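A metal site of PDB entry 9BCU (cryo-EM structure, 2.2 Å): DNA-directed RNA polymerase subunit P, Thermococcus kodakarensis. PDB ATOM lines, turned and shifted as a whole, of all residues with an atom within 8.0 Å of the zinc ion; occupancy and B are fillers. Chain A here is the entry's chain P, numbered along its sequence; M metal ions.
The nearest printed residue that does not touch the zinc ion is Ser 32 (4.5 Å).
The backbone NH of Lys 13 sits close to the side-chain sulfur of Cys 11 (3.2 Å). SG of Cys 27 lies close to N of Tyr 29 (3.4 Å). SG of Cys 8 lies close to OG of Ser 32, at 3.6 Å. The backbone NH (N) of Cys 8 lies within hydrogen-bond range of the backbone carbonyl oxygen (O) of Lys 13, 3.2 Å away. The side-chain sulfur (SG) of Cys 8 lies close to the backbone NH (N) of Lys 10, at 3.8 Å. O of Ser 32 sits at hydrogen-bond distance from N of Cys 27.
The zinc ion is bound by SG of Cys 11 (2.3 Å), SG of Cys 8 (2.3 Å), SG of Cys 27 (2.3 Å) and SG of Cys 30 (2.3 Å). The zinc ion has four donor atoms within binding distance.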
ATOM      1  N   ARG A   7      32.904  -6.435  23.222  1.00  0.00           N
ATOM      2  CA  ARG A   7      31.992  -5.302  23.274  1.00  0.00           C
ATOM      3  C   ARG A   7      30.863  -5.500  22.276  1.00  0.00           C
ATOM      4  O   ARG A   7      31.101  -5.902  21.130  1.00  0.00           O
ATOM      5  CB  ARG A   7      32.723  -3.988  22.973  1.00  0.00           C
ATOM      6  CG  ARG A   7      33.784  -3.614  23.993  1.00  0.00           C
ATOM      7  CD  ARG A   7      33.160  -3.029  25.246  1.00  0.00           C
ATOM      8  NE  ARG A   7      32.580  -1.705  25.002  1.00  0.00           N
ATOM      9  CZ  ARG A   7      33.269  -0.579  24.978  1.00  0.00           C
ATOM     10  NH1 ARG A   7      34.582  -0.561  25.189  1.00  0.00           N
ATOM     11  NH2 ARG A   7      32.635   0.565  24.750  1.00  0.00           N
ATOM     12  N   CYS A   8      29.637  -5.241  22.712  1.00  0.00           N
ATOM     13  CA  CYS A   8      28.484  -5.385  21.834  1.00  0.00           C
ATOM     14  C   CYS A   8      28.474  -4.275  20.783  1.00  0.00           C
ATOM     15  O   CYS A   8      28.901  -3.144  21.019  1.00  0.00           O
ATOM     16  CB  CYS A   8      27.189  -5.344  22.637  1.00  0.00           C
ATOM     17  SG  CYS A   8      25.744  -5.906  21.704  1.00  0.00           S
ATOM     18  N   ALA A   9      27.979  -4.632  19.587  1.00  0.00           N
ATOM     19  CA  ALA A   9      27.941  -3.669  18.494  1.00  0.00           C
ATOM     20  C   ALA A   9      26.831  -2.643  18.668  1.00  0.00           C
ATOM     21  O   ALA A   9      27.004  -1.478  18.314  1.00  0.00           O
ATOM     22  CB  ALA A   9      27.779  -4.410  17.158  1.00  0.00           C
ATOM     23  N   LYS A  10      25.684  -3.060  19.203  1.00  0.00           N
ATOM     24  CA  LYS A  10      24.526  -2.166  19.320  1.00  0.00           C
ATOM     25  C   LYS A  10      24.481  -1.465  20.679  1.00  0.00           C
ATOM     26  O   LYS A  10      24.526  -0.235  20.741  1.00  0.00           O
ATOM     27  CB  LYS A  10      23.240  -2.955  19.080  1.00  0.00           C
ATOM     28  CG  LYS A  10      23.332  -3.971  17.956  1.00  0.00           C
ATOM     29  CD  LYS A  10      21.953  -4.436  17.515  1.00  0.00           C
ATOM     30  CE  LYS A  10      21.944  -4.886  16.066  1.00  0.00           C
ATOM     31  NZ  LYS A  10      22.921  -5.981  15.822  1.00  0.00           N
ATOM     32  N   CYS A  11      24.393  -2.236  21.763  1.00  0.00           N
ATOM     33  CA  CYS A  11      24.295  -1.637  23.089  1.00  0.00           C
ATOM     34  C   CYS A  11      25.633  -1.097  23.566  1.00  0.00           C
ATOM     35  O   CYS A  11      25.657  -0.100  24.311  1.00  0.00           O
ATOM     36  CB  CYS A  11      23.749  -2.658  24.086  1.00  0.00           C
ATOM     37  SG  CYS A  11      24.979  -3.819  24.741  1.00  0.00           S
ATOM     38  N   GLY A  12      26.738  -1.706  23.163  1.00  0.00           N
ATOM     39  CA  GLY A  12      28.057  -1.242  23.531  1.00  0.00           C
ATOM     40  C   GLY A  12      28.547  -1.692  24.892  1.00  0.00           C
ATOM     41  O   GLY A  12      29.684  -1.346  25.265  1.00  0.00           O
ATOM     42  N   LYS A  13      27.750  -2.439  25.645  1.00  0.00           N
ATOM     43  CA  LYS A  13      28.174  -2.902  26.957  1.00  0.00           C
ATOM     44  C   LYS A  13      29.097  -4.106  26.831  1.00  0.00           C
ATOM     45  O   LYS A  13      29.112  -4.816  25.818  1.00  0.00           O
ATOM     46  CB  LYS A  13      26.949  -3.231  27.819  1.00  0.00           C
ATOM     47  CG  LYS A  13      26.281  -1.991  28.406  1.00  0.00           C
ATOM     48  CD  LYS A  13      24.780  -2.191  28.623  1.00  0.00           C
ATOM     49  CE  LYS A  13      24.486  -3.277  29.655  1.00  0.00           C
ATOM     50  NZ  LYS A  13      25.503  -3.347  30.730  1.00  0.00           N
ATOM     51  N   GLU A  14      29.860  -4.348  27.897  1.00  0.00           N
ATOM     52  CA  GLU A  14      30.871  -5.396  27.883  1.00  0.00           C
ATOM     53  C   GLU A  14      30.215  -6.777  27.965  1.00  0.00           C
ATOM     54  O   GLU A  14      29.328  -6.997  28.792  1.00  0.00           O
ATOM     55  CB  GLU A  14      31.842  -5.201  29.040  1.00  0.00           C
ATOM     56  CG  GLU A  14      33.272  -4.907  28.608  1.00  0.00           C
ATOM     57  CD  GLU A  14      34.125  -4.404  29.754  1.00  0.00           C
ATOM     58  OE1 GLU A  14      33.741  -3.412  30.396  1.00  0.00           O
ATOM     59  OE2 GLU A  14      35.187  -5.010  30.011  1.00  0.00           O
ATOM     60  N   VAL A  15      30.654  -7.689  27.100  1.00  0.00           N
ATOM     61  CA  VAL A  15      30.151  -9.061  27.064  1.00  0.00           C
ATOM     62  C   VAL A  15      31.331 -10.013  27.208  1.00  0.00           C
ATOM     63  O   VAL A  15      32.301  -9.917  26.462  1.00  0.00           O
ATOM     64  CB  VAL A  15      29.374  -9.341  25.759  1.00  0.00           C
ATOM     65  CG1 VAL A  15      28.953 -10.802  25.699  1.00  0.00           C
ATOM     66  CG2 VAL A  15      28.167  -8.430  25.652  1.00  0.00           C
ATOM     67  N   ARG A  26      25.892 -14.224  21.435  1.00  0.00           N
ATOM     68  CA  ARG A  26      24.905 -13.167  21.527  1.00  0.00           C
ATOM     69  C   ARG A  26      25.165 -12.351  22.789  1.00  0.00           C
ATOM     70  O   ARG A  26      25.816 -12.811  23.731  1.00  0.00           O
ATOM     71  CB  ARG A  26      23.475 -13.722  21.532  1.00  0.00           C
ATOM     72  CG  ARG A  26      22.928 -14.049  22.909  1.00  0.00           C
ATOM     73  CD  ARG A  26      21.484 -14.532  22.825  1.00  0.00           C
ATOM     74  NE  ARG A  26      20.536 -13.501  23.231  1.00  0.00           N
ATOM     75  CZ  ARG A  26      20.166 -13.273  24.482  1.00  0.00           C
ATOM     76  NH1 ARG A  26      20.649 -13.978  25.491  1.00  0.00           N
ATOM     77  NH2 ARG A  26      19.293 -12.300  24.724  1.00  0.00           N
ATOM     78  N   CYS A  27      24.645 -11.131  22.794  1.00  0.00           N
ATOM     79  CA  CYS A  27      24.760 -10.261  23.948  1.00  0.00           C
ATOM     80  C   CYS A  27      23.644 -10.572  24.945  1.00  0.00           C
ATOM     81  O   CYS A  27      22.468 -10.535  24.570  1.00  0.00           O
ATOM     82  CB  CYS A  27      24.703  -8.792  23.534  1.00  0.00           C
ATOM     83  SG  CYS A  27      24.616  -7.626  24.907  1.00  0.00           S
ATOM     84  N   PRO A  28      23.958 -10.883  26.200  1.00  0.00           N
ATOM     85  CA  PRO A  28      22.908 -11.209  27.174  1.00  0.00           C
ATOM     86  C   PRO A  28      22.065 -10.009  27.581  1.00  0.00           C
ATOM     87  O   PRO A  28      21.041 -10.198  28.265  1.00  0.00           O
ATOM     88  CB  PRO A  28      23.682 -11.767  28.367  1.00  0.00           C
ATOM     89  CG  PRO A  28      25.028 -11.115  28.267  1.00  0.00           C
ATOM     90  CD  PRO A  28      25.305 -10.940  26.798  1.00  0.00           C
ATOM     91  N   TYR A  29      22.435  -8.797  27.198  1.00  0.00           N
ATOM     92  CA  TYR A  29      21.728  -7.593  27.618  1.00  0.00           C
ATOM     93  C   TYR A  29      20.658  -7.173  26.626  1.00  0.00           C
ATOM     94  O   TYR A  29      19.517  -6.880  27.020  1.00  0.00           O
ATOM     95  CB  TYR A  29      22.733  -6.452  27.849  1.00  0.00           C
ATOM     96  CG  TYR A  29      23.802  -6.800  28.861  1.00  0.00           C
ATOM     97  CD1 TYR A  29      23.473  -7.381  30.068  1.00  0.00           C
ATOM     98  CD2 TYR A  29      25.140  -6.559  28.589  1.00  0.00           C
ATOM     99  CE1 TYR A  29      24.458  -7.702  30.998  1.00  0.00           C
ATOM    100  CE2 TYR A  29      26.127  -6.865  29.503  1.00  0.00           C
ATOM    101  CZ  TYR A  29      25.775  -7.437  30.708  1.00  0.00           C
ATOM    102  OH  TYR A  29      26.751  -7.751  31.631  1.00  0.00           O
ATOM    103  N   CYS A  30      20.990  -7.116  25.340  1.00  0.00           N
ATOM    104  CA  CYS A  30      20.051  -6.689  24.313  1.00  0.00           C
ATOM    105  C   CYS A  30      19.764  -7.748  23.262  1.00  0.00           C
ATOM    106  O   CYS A  30      18.918  -7.512  22.390  1.00  0.00           O
ATOM    107  CB  CYS A  30      20.566  -5.412  23.626  1.00  0.00           C
ATOM    108  SG  CYS A  30      22.166  -5.584  22.812  1.00  0.00           S
ATOM    109  N   GLY A  31      20.447  -8.894  23.305  1.00  0.00           N
ATOM    110  CA  GLY A  31      20.177  -9.965  22.359  1.00  0.00           C
ATOM    111  C   GLY A  31      20.871  -9.835  21.026  1.00  0.00           C
ATOM    112  O   GLY A  31      20.603 -10.641  20.126  1.00  0.00           O
ATOM    113  N   SER A  32      21.748  -8.850  20.849  1.00  0.00           N
ATOM    114  CA  SER A  32      22.450  -8.682  19.587  1.00  0.00           C
ATOM    115  C   SER A  32      23.463  -9.813  19.383  1.00  0.00           C
ATOM    116  O   SER A  32      24.189 -10.188  20.307  1.00  0.00           O
ATOM    117  CB  SER A  32      23.155  -7.338  19.540  1.00  0.00           C
ATOM    118  OG  SER A  32      24.342  -7.403  18.777  1.00  0.00           O
ATOM    119  N   LYS A  33      23.503 -10.341  18.168  1.00  0.00           N
ATOM    120  CA  LYS A  33      24.408 -11.428  17.820  1.00  0.00           C
ATOM    121  C   LYS A  33      25.714 -10.954  17.209  1.00  0.00           C
ATOM    122  O   LYS A  33      26.536 -11.786  16.814  1.00  0.00           O
ATOM    123  CB  LYS A  33      23.716 -12.395  16.863  1.00  0.00           C
ATOM    124  CG  LYS A  33      22.443 -13.009  17.411  1.00  0.00           C
ATOM    125  CD  LYS A  33      22.663 -14.440  17.863  1.00  0.00           C
ATOM    126  CE  LYS A  33      23.127 -15.312  16.707  1.00  0.00           C
ATOM    127  NZ  LYS A  33      23.009 -16.766  17.025  1.00  0.00           N
ATOM    128  N   ILE A  34      25.931  -9.643  17.114  1.00  0.00           N
ATOM    129  CA  ILE A  34      27.155  -9.072  16.548  1.00  0.00           C
ATOM    130  C   ILE A  34      27.937  -8.409  17.675  1.00  0.00           C
ATOM    131  O   ILE A  34      27.400  -7.567  18.404  1.00  0.00           O
ATOM    132  CB  ILE A  34      26.830  -8.063  15.435  1.00  0.00           C
ATOM    133  CG1 ILE A  34      26.053  -8.738  14.304  1.00  0.00           C
ATOM    134  CG2 ILE A  34      28.108  -7.434  14.897  1.00  0.00           C
ATOM    135  CD1 ILE A  34      25.169  -7.793  13.524  1.00  0.00           C
ATOM    136  N   LEU A  35      29.201  -8.806  17.824  1.00  0.00           N
ATOM    137  CA  LEU A  35      30.056  -8.304  18.879  1.00  0.00           C
ATOM    138  C   LEU A  35      31.346  -7.748  18.291  1.00  0.00           C
ATOM    139  O   LEU A  35      31.757  -8.119  17.189  1.00  0.00           O
ATOM    140  CB  LEU A  35      30.387  -9.398  19.909  1.00  0.00           C
ATOM    141  CG  LEU A  35      29.198 -10.109  20.551  1.00  0.00           C
ATOM    142  CD1 LEU A  35      29.682 -11.240  21.456  1.00  0.00           C
ATOM    143  CD2 LEU A  35      28.336  -9.130  21.338  1.00  0.00           C
HETATM  144 ZN    ZN M   1      24.365  -5.730  23.575  1.00  0.00          ZN
